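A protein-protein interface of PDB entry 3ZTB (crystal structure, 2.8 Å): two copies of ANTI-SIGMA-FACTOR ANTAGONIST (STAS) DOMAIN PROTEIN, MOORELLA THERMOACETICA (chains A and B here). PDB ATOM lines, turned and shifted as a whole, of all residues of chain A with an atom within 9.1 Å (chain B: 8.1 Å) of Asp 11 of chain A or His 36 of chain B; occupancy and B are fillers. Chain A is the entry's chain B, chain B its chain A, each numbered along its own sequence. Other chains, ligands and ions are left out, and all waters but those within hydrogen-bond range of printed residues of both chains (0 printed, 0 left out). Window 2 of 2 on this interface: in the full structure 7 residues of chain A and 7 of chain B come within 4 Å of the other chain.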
ATOM      1  N   LEU A   8      27.588  -4.359 -23.594  1.00  0.00           N
ATOM      2  CA  LEU A   8      27.034  -3.358 -24.498  1.00  0.00           C
ATOM      3  C   LEU A   8      28.118  -2.362 -24.927  1.00  0.00           C
ATOM      4  O   LEU A   8      29.188  -2.300 -24.315  1.00  0.00           O
ATOM      5  CB  LEU A   8      25.869  -2.631 -23.824  1.00  0.00           C
ATOM      6  CG  LEU A   8      24.843  -3.529 -23.136  1.00  0.00           C
ATOM      7  CD1 LEU A   8      23.939  -2.732 -22.208  1.00  0.00           C
ATOM      8  CD2 LEU A   8      24.013  -4.299 -24.153  1.00  0.00           C
ATOM      9  N   LYS A   9      27.850  -1.590 -25.979  1.00  0.00           N
ATOM     10  CA  LYS A   9      28.804  -0.585 -26.452  1.00  0.00           C
ATOM     11  C   LYS A   9      28.106   0.536 -27.206  1.00  0.00           C
ATOM     12  O   LYS A   9      27.467   0.304 -28.232  1.00  0.00           O
ATOM     13  CB  LYS A   9      29.869  -1.204 -27.362  1.00  0.00           C
ATOM     14  CG  LYS A   9      30.646  -0.192 -28.207  1.00  0.00           C
ATOM     15  CD  LYS A   9      32.138  -0.309 -27.933  1.00  0.00           C
ATOM     16  CE  LYS A   9      32.941  -0.252 -29.225  1.00  0.00           C
ATOM     17  NZ  LYS A   9      34.421  -0.227 -28.991  1.00  0.00           N
ATOM     18  N   VAL A  10      28.224   1.752 -26.688  1.00  0.00           N
ATOM     19  CA  VAL A  10      27.674   2.925 -27.360  1.00  0.00           C
ATOM     20  C   VAL A  10      28.747   3.987 -27.560  1.00  0.00           C
ATOM     21  O   VAL A  10      29.355   4.443 -26.590  1.00  0.00           O
ATOM     22  CB  VAL A  10      26.496   3.505 -26.575  1.00  0.00           C
ATOM     23  CG1 VAL A  10      26.737   3.308 -25.088  1.00  0.00           C
ATOM     24  CG2 VAL A  10      26.317   4.992 -26.892  1.00  0.00           C
ATOM     25  N   ASP A  11      28.983   4.363 -28.819  1.00  0.00           N
ATOM     26  CA  ASP A  11      29.792   5.542 -29.144  1.00  0.00           C
ATOM     27  C   ASP A  11      31.299   5.377 -28.966  1.00  0.00           C
ATOM     28  O   ASP A  11      32.009   6.372 -28.826  1.00  0.00           O
ATOM     29  CB  ASP A  11      29.326   6.733 -28.298  1.00  0.00           C
ATOM     30  CG  ASP A  11      28.505   7.723 -29.085  1.00  0.00           C
ATOM     31  OD1 ASP A  11      28.289   7.476 -30.282  1.00  0.00           O
ATOM     32  OD2 ASP A  11      28.068   8.736 -28.506  1.00  0.00           O
ATOM     33  N   ASP A  12      31.777   4.137 -28.974  1.00  0.00           N
ATOM     34  CA  ASP A  12      33.181   3.833 -28.679  1.00  0.00           C
ATOM     35  C   ASP A  12      33.354   3.586 -27.188  1.00  0.00           C
ATOM     36  O   ASP A  12      34.465   3.381 -26.705  1.00  0.00           O
ATOM     37  CB  ASP A  12      34.114   4.974 -29.117  1.00  0.00           C
ATOM     38  CG  ASP A  12      34.807   4.711 -30.443  1.00  0.00           C
ATOM     39  OD1 ASP A  12      34.789   3.562 -30.919  1.00  0.00           O
ATOM     40  OD2 ASP A  12      35.377   5.672 -31.003  1.00  0.00           O
ATOM     41  N   TYR A  13      32.241   3.620 -26.466  1.00  0.00           N
ATOM     42  CA  TYR A  13      32.255   3.425 -25.024  1.00  0.00           C
ATOM     43  C   TYR A  13      31.668   2.071 -24.638  1.00  0.00           C
ATOM     44  O   TYR A  13      30.534   1.750 -24.995  1.00  0.00           O
ATOM     45  CB  TYR A  13      31.495   4.552 -24.321  1.00  0.00           C
ATOM     46  CG  TYR A  13      32.216   5.881 -24.343  1.00  0.00           C
ATOM     47  CD1 TYR A  13      33.186   6.179 -23.397  1.00  0.00           C
ATOM     48  CD2 TYR A  13      31.933   6.834 -25.313  1.00  0.00           C
ATOM     49  CE1 TYR A  13      33.852   7.390 -23.412  1.00  0.00           C
ATOM     50  CE2 TYR A  13      32.595   8.049 -25.335  1.00  0.00           C
ATOM     51  CZ  TYR A  13      33.553   8.321 -24.382  1.00  0.00           C
ATOM     52  OH  TYR A  13      34.213   9.528 -24.403  1.00  0.00           O
ATOM     53  N   TRP A  14      32.454   1.280 -23.916  1.00  0.00           N
ATOM     54  CA  TRP A  14      32.006  -0.019 -23.434  1.00  0.00           C
ATOM     55  C   TRP A  14      31.110   0.145 -22.216  1.00  0.00           C
ATOM     56  O   TRP A  14      31.368   0.983 -21.352  1.00  0.00           O
ATOM     57  CB  TRP A  14      33.207  -0.896 -23.079  1.00  0.00           C
ATOM     58  CG  TRP A  14      34.083  -1.212 -24.249  1.00  0.00           C
ATOM     59  CD1 TRP A  14      35.324  -0.706 -24.510  1.00  0.00           C
ATOM     60  CD2 TRP A  14      33.780  -2.106 -25.327  1.00  0.00           C
ATOM     61  NE1 TRP A  14      35.813  -1.233 -25.682  1.00  0.00           N
ATOM     62  CE2 TRP A  14      34.884  -2.095 -26.201  1.00  0.00           C
ATOM     63  CE3 TRP A  14      32.683  -2.914 -25.632  1.00  0.00           C
ATOM     64  CZ2 TRP A  14      34.919  -2.864 -27.365  1.00  0.00           C
ATOM     65  CZ3 TRP A  14      32.720  -3.675 -26.784  1.00  0.00           C
ATOM     66  CH2 TRP A  14      33.830  -3.645 -27.636  1.00  0.00           C
ATOM     67  N   VAL A  15      30.056  -0.662 -22.145  1.00  0.00           N
ATOM     68  CA  VAL A  15      29.124  -0.596 -21.025  1.00  0.00           C
ATOM     69  C   VAL A  15      28.879  -1.972 -20.421  1.00  0.00           C
ATOM     70  O   VAL A  15      28.322  -2.854 -21.074  1.00  0.00           O
ATOM     71  CB  VAL A  15      27.769  -0.003 -21.443  1.00  0.00           C
ATOM     72  CG1 VAL A  15      26.822   0.066 -20.250  1.00  0.00           C
ATOM     73  CG2 VAL A  15      27.958   1.375 -22.055  1.00  0.00           C
ATOM     74  N   ALA A  42      39.959  -1.514 -28.738  1.00  0.00           N
ATOM     75  CA  ALA A  42      39.949  -0.606 -27.594  1.00  0.00           C
ATOM     76  C   ALA A  42      38.794   0.393 -27.684  1.00  0.00           C
ATOM     77  O   ALA A  42      38.227   0.619 -28.755  1.00  0.00           O
ATOM     78  CB  ALA A  42      41.270   0.122 -27.482  1.00  0.00           C
ATOM     79  N   GLY A  43      38.459   0.998 -26.552  1.00  0.00           N
ATOM     80  CA  GLY A  43      37.402   1.989 -26.505  1.00  0.00           C
ATOM     81  C   GLY A  43      37.888   3.291 -25.904  1.00  0.00           C
ATOM     82  O   GLY A  43      38.994   3.356 -25.372  1.00  0.00           O
ATOM     83  N   LYS A  44      37.065   4.331 -25.989  1.00  0.00           N
ATOM     84  CA  LYS A  44      37.403   5.607 -25.367  1.00  0.00           C
ATOM     85  C   LYS A  44      37.085   5.622 -23.876  1.00  0.00           C
ATOM     86  O   LYS A  44      37.315   6.628 -23.207  1.00  0.00           O
ATOM     87  CB  LYS A  44      36.675   6.772 -26.044  1.00  0.00           C
ATOM     88  CG  LYS A  44      37.187   7.138 -27.424  1.00  0.00           C
ATOM     89  CD  LYS A  44      36.855   8.589 -27.752  1.00  0.00           C
ATOM     90  CE  LYS A  44      37.315   8.963 -29.154  1.00  0.00           C
ATOM     91  NZ  LYS A  44      37.091  10.407 -29.457  1.00  0.00           N
ATOM     92  N   GLY A  45      36.553   4.519 -23.356  1.00  0.00           N
ATOM     93  CA  GLY A  45      36.098   4.482 -21.978  1.00  0.00           C
ATOM     94  C   GLY A  45      35.265   3.269 -21.613  1.00  0.00           C
ATOM     95  O   GLY A  45      34.973   2.416 -22.452  1.00  0.00           O
ATOM     96  N   GLN A 108      23.396   7.559 -18.889  1.00  0.00           N
ATOM     97  CA  GLN A 108      23.387   8.784 -19.688  1.00  0.00           C
ATOM     98  C   GLN A 108      24.336   9.854 -19.147  1.00  0.00           C
ATOM     99  O   GLN A 108      25.165  10.386 -19.885  1.00  0.00           O
ATOM    100  CB  GLN A 108      21.969   9.357 -19.759  1.00  0.00           C
ATOM    101  CG  GLN A 108      21.828  10.571 -20.664  1.00  0.00           C
ATOM    102  CD  GLN A 108      21.554  10.196 -22.106  1.00  0.00           C
ATOM    103  OE1 GLN A 108      22.454  10.211 -22.946  1.00  0.00           O
ATOM    104  NE2 GLN A 108      20.304   9.857 -22.402  1.00  0.00           N
ATOM    105  N   LEU A 111      27.832   8.720 -19.574  1.00  0.00           N
ATOM    106  CA  LEU A 111      28.266   8.863 -20.959  1.00  0.00           C
ATOM    107  C   LEU A 111      28.588  10.323 -21.257  1.00  0.00           C
ATOM    108  O   LEU A 111      29.565  10.627 -21.941  1.00  0.00           O
ATOM    109  CB  LEU A 111      27.206   8.335 -21.930  1.00  0.00           C
ATOM    110  CG  LEU A 111      27.132   6.818 -22.113  1.00  0.00           C
ATOM    111  CD1 LEU A 111      25.919   6.432 -22.947  1.00  0.00           C
ATOM    112  CD2 LEU A 111      28.409   6.282 -22.744  1.00  0.00           C
ATOM    113  N   ASP A 112      27.768  11.223 -20.725  1.00  0.00           N
ATOM    114  CA  ASP A 112      27.986  12.654 -20.902  1.00  0.00           C
ATOM    115  C   ASP A 112      29.264  13.119 -20.208  1.00  0.00           C
ATOM    116  O   ASP A 112      29.965  13.994 -20.709  1.00  0.00           O
ATOM    117  CB  ASP A 112      26.782  13.453 -20.398  1.00  0.00           C
ATOM    118  CG  ASP A 112      25.548  13.256 -21.260  1.00  0.00           C
ATOM    119  OD1 ASP A 112      25.689  12.779 -22.407  1.00  0.00           O
ATOM    120  OD2 ASP A 112      24.438  13.585 -20.794  1.00  0.00           O
ATOM    121  N   LEU A 114      31.977  11.199 -19.532  1.00  0.00           N
ATOM    122  CA  LEU A 114      33.115  10.594 -20.224  1.00  0.00           C
ATOM    123  C   LEU A 114      33.503  11.285 -21.538  1.00  0.00           C
ATOM    124  O   LEU A 114      34.634  11.159 -21.988  1.00  0.00           O
ATOM    125  CB  LEU A 114      32.874   9.098 -20.460  1.00  0.00           C
ATOM    126  CG  LEU A 114      33.220   8.148 -19.317  1.00  0.00           C
ATOM    127  CD1 LEU A 114      33.596   6.783 -19.868  1.00  0.00           C
ATOM    128  CD2 LEU A 114      34.362   8.712 -18.477  1.00  0.00           C
ATOM    129  N   LYS A 115      32.571  12.018 -22.140  1.00  0.00           N
ATOM    130  CA  LYS A 115      32.812  12.660 -23.432  1.00  0.00           C
ATOM    131  C   LYS A 115      32.789  14.184 -23.381  1.00  0.00           C
ATOM    132  O   LYS A 115      33.577  14.838 -24.063  1.00  0.00           O
ATOM    133  CB  LYS A 115      31.808  12.151 -24.457  1.00  0.00           C
ATOM    134  CG  LYS A 115      30.373  12.541 -24.133  1.00  0.00           C
ATOM    135  CD  LYS A 115      29.420  11.548 -24.764  1.00  0.00           C
ATOM    136  CE  LYS A 115      29.812  11.267 -26.184  1.00  0.00           C
ATOM    137  NZ  LYS A 115      28.852  10.346 -26.821  1.00  0.00           N
ATOM    138  N   ASN A 116      31.868  14.747 -22.606  1.00  0.00           N
ATOM    139  CA  ASN A 116      31.857  16.183 -22.349  1.00  0.00           C
ATOM    140  C   ASN A 116      33.025  16.531 -21.439  1.00  0.00           C
ATOM    141  O   ASN A 116      33.016  17.533 -20.736  1.00  0.00           O
ATOM    142  CB  ASN A 116      30.525  16.622 -21.719  1.00  0.00           C
ATOM    143  CG  ASN A 116      29.478  17.011 -22.750  1.00  0.00           C
ATOM    144  OD1 ASN A 116      29.217  18.197 -22.969  1.00  0.00           O
ATOM    145  ND2 ASN A 116      28.870  16.016 -23.382  1.00  0.00           N
ATOM    146  N   ILE B   7      16.303   6.574 -39.770  1.00  0.00           N
ATOM    147  CA  ILE B   7      15.847   6.841 -38.414  1.00  0.00           C
ATOM    148  C   ILE B   7      15.041   8.133 -38.411  1.00  0.00           C
ATOM    149  O   ILE B   7      15.571   9.217 -38.661  1.00  0.00           O
ATOM    150  CB  ILE B   7      17.019   6.963 -37.427  1.00  0.00           C
ATOM    151  CG1 ILE B   7      17.755   5.631 -37.330  1.00  0.00           C
ATOM    152  CG2 ILE B   7      16.515   7.405 -36.061  1.00  0.00           C
ATOM    153  CD1 ILE B   7      19.250   5.768 -37.249  1.00  0.00           C
ATOM    154  N   TRP B  14      11.379   8.310 -31.279  1.00  0.00           N
ATOM    155  CA  TRP B  14      12.221   7.722 -32.310  1.00  0.00           C
ATOM    156  C   TRP B  14      11.455   6.626 -33.044  1.00  0.00           C
ATOM    157  O   TRP B  14      10.858   5.750 -32.417  1.00  0.00           O
ATOM    158  CB  TRP B  14      13.520   7.173 -31.716  1.00  0.00           C
ATOM    159  CG  TRP B  14      14.391   8.224 -31.096  1.00  0.00           C
ATOM    160  CD1 TRP B  14      14.559   8.469 -29.763  1.00  0.00           C
ATOM    161  CD2 TRP B  14      15.212   9.173 -31.781  1.00  0.00           C
ATOM    162  NE1 TRP B  14      15.433   9.511 -29.577  1.00  0.00           N
ATOM    163  CE2 TRP B  14      15.852   9.965 -30.811  1.00  0.00           C
ATOM    164  CE3 TRP B  14      15.473   9.438 -33.133  1.00  0.00           C
ATOM    165  CZ2 TRP B  14      16.730  10.994 -31.129  1.00  0.00           C
ATOM    166  CZ3 TRP B  14      16.346  10.460 -33.455  1.00  0.00           C
ATOM    167  CH2 TRP B  14      16.963  11.226 -32.459  1.00  0.00           C
ATOM    168  N   GLN B  29      25.859  -0.183 -38.961  1.00  0.00           N
ATOM    169  CA  GLN B  29      25.813   1.247 -39.248  1.00  0.00           C
ATOM    170  C   GLN B  29      24.551   1.845 -38.637  1.00  0.00           C
ATOM    171  O   GLN B  29      24.563   2.964 -38.128  1.00  0.00           O
ATOM    172  CB  GLN B  29      25.850   1.502 -40.755  1.00  0.00           C
ATOM    173  CG  GLN B  29      25.737   2.973 -41.152  1.00  0.00           C
ATOM    174  CD  GLN B  29      25.466   3.149 -42.635  1.00  0.00           C
ATOM    175  OE1 GLN B  29      25.251   2.173 -43.355  1.00  0.00           O
ATOM    176  NE2 GLN B  29      25.471   4.394 -43.100  1.00  0.00           N
ATOM    177  N   PHE B  30      23.468   1.076 -38.688  1.00  0.00           N
ATOM    178  CA  PHE B  30      22.182   1.479 -38.130  1.00  0.00           C
ATOM    179  C   PHE B  30      22.205   1.529 -36.602  1.00  0.00           C
ATOM    180  O   PHE B  30      21.829   2.534 -35.997  1.00  0.00           O
ATOM    181  CB  PHE B  30      21.086   0.518 -38.601  1.00  0.00           C
ATOM    182  CG  PHE B  30      19.980   0.335 -37.610  1.00  0.00           C
ATOM    183  CD1 PHE B  30      19.056   1.342 -37.397  1.00  0.00           C
ATOM    184  CD2 PHE B  30      19.866  -0.841 -36.885  1.00  0.00           C
ATOM    185  CE1 PHE B  30      18.038   1.183 -36.481  1.00  0.00           C
ATOM    186  CE2 PHE B  30      18.848  -1.006 -35.967  1.00  0.00           C
ATOM    187  CZ  PHE B  30      17.933   0.008 -35.766  1.00  0.00           C
ATOM    188  N   LYS B  31      22.638   0.431 -35.989  1.00  0.00           N
ATOM    189  CA  LYS B  31      22.731   0.320 -34.533  1.00  0.00           C
ATOM    190  C   LYS B  31      23.626   1.395 -33.927  1.00  0.00           C
ATOM    191  O   LYS B  31      23.244   2.063 -32.964  1.00  0.00           O
ATOM    192  CB  LYS B  31      23.263  -1.060 -34.136  1.00  0.00           C
ATOM    193  CG  LYS B  31      23.620  -1.193 -32.660  1.00  0.00           C
ATOM    194  CD  LYS B  31      24.323  -2.513 -32.373  1.00  0.00           C
ATOM    195  CE  LYS B  31      25.708  -2.561 -33.006  1.00  0.00           C
ATOM    196  NZ  LYS B  31      26.263  -3.946 -33.017  1.00  0.00           N
ATOM    197  N   GLU B  32      24.826   1.545 -34.480  1.00  0.00           N
ATOM    198  CA  GLU B  32      25.756   2.560 -34.003  1.00  0.00           C
ATOM    199  C   GLU B  32      25.128   3.932 -34.136  1.00  0.00           C
ATOM    200  O   GLU B  32      25.209   4.761 -33.231  1.00  0.00           O
ATOM    201  CB  GLU B  32      27.052   2.528 -34.811  1.00  0.00           C
ATOM    202  CG  GLU B  32      27.928   1.317 -34.596  1.00  0.00           C
ATOM    203  CD  GLU B  32      29.281   1.490 -35.252  1.00  0.00           C
ATOM    204  OE1 GLU B  32      29.368   2.278 -36.217  1.00  0.00           O
ATOM    205  OE2 GLU B  32      30.257   0.861 -34.796  1.00  0.00           O
ATOM    206  N   GLU B  33      24.503   4.162 -35.282  1.00  0.00           N
ATOM    207  CA  GLU B  33      23.850   5.431 -35.551  1.00  0.00           C
ATOM    208  C   GLU B  33      22.662   5.654 -34.620  1.00  0.00           C
ATOM    209  O   GLU B  33      22.480   6.757 -34.109  1.00  0.00           O
ATOM    210  CB  GLU B  33      23.395   5.502 -37.008  1.00  0.00           C
ATOM    211  CG  GLU B  33      22.989   6.885 -37.458  1.00  0.00           C
ATOM    212  CD  GLU B  33      22.408   6.892 -38.854  1.00  0.00           C
ATOM    213  OE1 GLU B  33      22.275   5.805 -39.457  1.00  0.00           O
ATOM    214  OE2 GLU B  33      22.083   7.990 -39.347  1.00  0.00           O
ATOM    215  N   LEU B  34      21.855   4.618 -34.391  1.00  0.00           N
ATOM    216  CA  LEU B  34      20.681   4.763 -33.533  1.00  0.00           C
ATOM    217  C   LEU B  34      21.104   5.074 -32.105  1.00  0.00           C
ATOM    218  O   LEU B  34      20.640   6.043 -31.507  1.00  0.00           O
ATOM    219  CB  LEU B  34      19.803   3.507 -33.560  1.00  0.00           C
ATOM    220  CG  LEU B  34      18.536   3.566 -32.692  1.00  0.00           C
ATOM    221  CD1 LEU B  34      17.462   4.472 -33.292  1.00  0.00           C
ATOM    222  CD2 LEU B  34      17.971   2.175 -32.456  1.00  0.00           C
ATOM    223  N   LEU B  35      21.989   4.241 -31.570  1.00  0.00           N
ATOM    224  CA  LEU B  35      22.494   4.410 -30.210  1.00  0.00           C
ATOM    225  C   LEU B  35      23.226   5.739 -30.018  1.00  0.00           C
ATOM    226  O   LEU B  35      23.318   6.247 -28.903  1.00  0.00           O
ATOM    227  CB  LEU B  35      23.403   3.240 -29.824  1.00  0.00           C
ATOM    228  CG  LEU B  35      22.700   1.882 -29.785  1.00  0.00           C
ATOM    229  CD1 LEU B  35      23.695   0.749 -29.589  1.00  0.00           C
ATOM    230  CD2 LEU B  35      21.652   1.881 -28.689  1.00  0.00           C
ATOM    231  N   HIS B  36      23.749   6.298 -31.104  1.00  0.00           N
ATOM    232  CA  HIS B  36      24.386   7.609 -31.041  1.00  0.00           C
ATOM    233  C   HIS B  36      23.315   8.684 -30.922  1.00  0.00           C
ATOM    234  O   HIS B  36      23.480   9.676 -30.211  1.00  0.00           O
ATOM    235  CB  HIS B  36      25.255   7.851 -32.277  1.00  0.00           C
ATOM    236  CG  HIS B  36      25.822   9.242 -32.359  1.00  0.00           C
ATOM    237  ND1 HIS B  36      26.528   9.813 -31.323  1.00  0.00           N
ATOM    238  CD2 HIS B  36      25.788  10.154 -33.344  1.00  0.00           C
ATOM    239  CE1 HIS B  36      26.904  11.030 -31.669  1.00  0.00           C
ATOM    240  NE2 HIS B  36      26.465  11.266 -32.903  1.00  0.00           N
ATOM    241  N   ASN B  37      22.207   8.462 -31.620  1.00  0.00           N
ATOM    242  CA  ASN B  37      21.083   9.390 -31.636  1.00  0.00           C
ATOM    243  C   ASN B  37      20.300   9.429 -30.317  1.00  0.00           C
ATOM    244  O   ASN B  37      19.999  10.504 -29.796  1.00  0.00           O
ATOM    245  CB  ASN B  37      20.150   9.050 -32.804  1.00  0.00           C
ATOM    246  CG  ASN B  37      20.656   9.586 -34.137  1.00  0.00           C
ATOM    247  OD1 ASN B  37      19.954  10.326 -34.820  1.00  0.00           O
ATOM    248  ND2 ASN B  37      21.881   9.226 -34.505  1.00  0.00           N
ATOM    249  N   ILE B  38      19.982   8.256 -29.778  1.00  0.00           N
ATOM    250  CA  ILE B  38      19.162   8.168 -28.570  1.00  0.00           C
ATOM    251  C   ILE B  38      19.939   8.523 -27.302  1.00  0.00           C
ATOM    252  O   ILE B  38      19.430   8.367 -26.191  1.00  0.00           O
ATOM    253  CB  ILE B  38      18.548   6.764 -28.397  1.00  0.00           C
ATOM    254  CG1 ILE B  38      19.607   5.768 -27.922  1.00  0.00           C
ATOM    255  CG2 ILE B  38      17.902   6.298 -29.693  1.00  0.00           C
ATOM    256  CD1 ILE B  38      19.083   4.358 -27.739  1.00  0.00           C
ATOM    257  N   THR B  39      21.169   8.996 -27.472  1.00  0.00           N
ATOM    258  CA  THR B  39      22.017   9.359 -26.341  1.00  0.00           C
ATOM    259  C   THR B  39      22.447  10.820 -26.399  1.00  0.00           C
ATOM    260  O   THR B  39      22.678  11.453 -25.368  1.00  0.00           O
ATOM    261  CB  THR B  39      23.276   8.479 -26.272  1.00  0.00           C
ATOM    262  OG1 THR B  39      23.975   8.539 -27.523  1.00  0.00           O
ATOM    263  CG2 THR B  39      22.904   7.036 -25.972  1.00  0.00           C
ATOM    264  N   GLY B  40      22.556  11.348 -27.614  1.00  0.00           N
ATOM    265  CA  GLY B  40      22.989  12.717 -27.818  1.00  0.00           C
ATOM    266  C   GLY B  40      21.938  13.754 -27.463  1.00  0.00           C
ATOM    267  O   GLY B  40      22.252  14.763 -26.830  1.00  0.00           O
ATOM    268  N   VAL B  41      20.692  13.514 -27.869  1.00  0.00           N
ATOM    269  CA  VAL B  41      19.609  14.466 -27.618  1.00  0.00           C
ATOM    270  C   VAL B  41      18.320  13.778 -27.136  1.00  0.00           C
ATOM    271  O   VAL B  41      18.052  12.629 -27.481  1.00  0.00           O
ATOM    272  CB  VAL B  41      19.329  15.340 -28.871  1.00  0.00           C
ATOM    273  CG1 VAL B  41      18.380  14.634 -29.827  1.00  0.00           C
ATOM    274  CG2 VAL B  41      18.776  16.694 -28.462  1.00  0.00           C
ATOM    275  N   LEU B  70      19.882  -1.233 -23.729  1.00  0.00           N
ATOM    276  CA  LEU B  70      20.464   0.100 -23.591  1.00  0.00           C
ATOM    277  C   LEU B  70      19.409   1.181 -23.387  1.00  0.00           C
ATOM    278  O   LEU B  70      19.666   2.183 -22.718  1.00  0.00           O
ATOM    279  CB  LEU B  70      21.364   0.443 -24.779  1.00  0.00           C
ATOM    280  CG  LEU B  70      22.801  -0.076 -24.668  1.00  0.00           C
ATOM    281  CD1 LEU B  70      23.557   0.128 -25.970  1.00  0.00           C
ATOM    282  CD2 LEU B  70      23.528   0.591 -23.508  1.00  0.00           C
ATOM    283  N   LEU B  74      18.735   3.815 -20.394  1.00  0.00           N
ATOM    284  CA  LEU B  74      18.600   5.247 -20.633  1.00  0.00           C
ATOM    285  C   LEU B  74      17.219   5.748 -20.218  1.00  0.00           C
ATOM    286  O   LEU B  74      16.920   6.937 -20.335  1.00  0.00           O
ATOM    287  CB  LEU B  74      18.856   5.569 -22.106  1.00  0.00           C
ATOM    288  CG  LEU B  74      20.254   5.266 -22.646  1.00  0.00           C
ATOM    289  CD1 LEU B  74      20.260   5.283 -24.167  1.00  0.00           C
ATOM    290  CD2 LEU B  74      21.276   6.246 -22.091  1.00  0.00           C
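Leu 8 of chain A touches Leu 70 of chain B. Val 10 of chain A touches Leu 35 of chain B (CG2 to O, 3.8 Å). Gln 108 of chain A touches Leu 74 of chain B.
Among the printed residues, no Asp or Glu carboxylate lies within 4 Å of a Lys or Arg side-chain nitrogen of the other chain.
Of the printed residues of chain B, Leu 8 of chain A touches Leu 70. Of the printed residues of chain B, Val 10 of chain A touches Leu 35. Printed residues of chain B within 4 Å of Asp 11 of chain A: His 36. Of the printed residues of chain A, Leu 35 of chain B touches Val 10. His 36 of chain B touches one residue of chain A. Asn 37 of chain B touches none of the printed residues of chain A. Of the printed residues of chain A, Thr 39 of chain B touches Gln 108.
The side-chain amino group (NZ) of Lys 115 of chain A is in salt-bridge range of the side-chain carboxylate (OD2) of Asp 11 of chain A (2.5 Å). The backbone carbonyl oxygen (O) of Leu 35 of chain B is in hydrogen-bond range of the side-chain hydroxyl (OG1) of Thr 39 of chain B. The side-chain hydroxyl of Thr 39 of chain B lies within hydrogen-bond range of the backbone carbonyl oxygen of His 36 of chain B (3.0 Å). The backbone carbonyl oxygen of Leu 8 of chain A is in hydrogen-bond range of the backbone NH of Val 15 of chain A.
The side-chain amide oxygen (OE1) of Gln 108 of chain A sits close to the backbone carbonyl oxygen (O) of Thr 39 of chain B (2.7 Å). The side-chain carboxylate (OD1) of Asp 11 of chain A is in hydrogen-bond range of a ring nitrogen (ND1) of His 36 of chain B, at 3.1 Å.
Position printed for both chains: 14.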
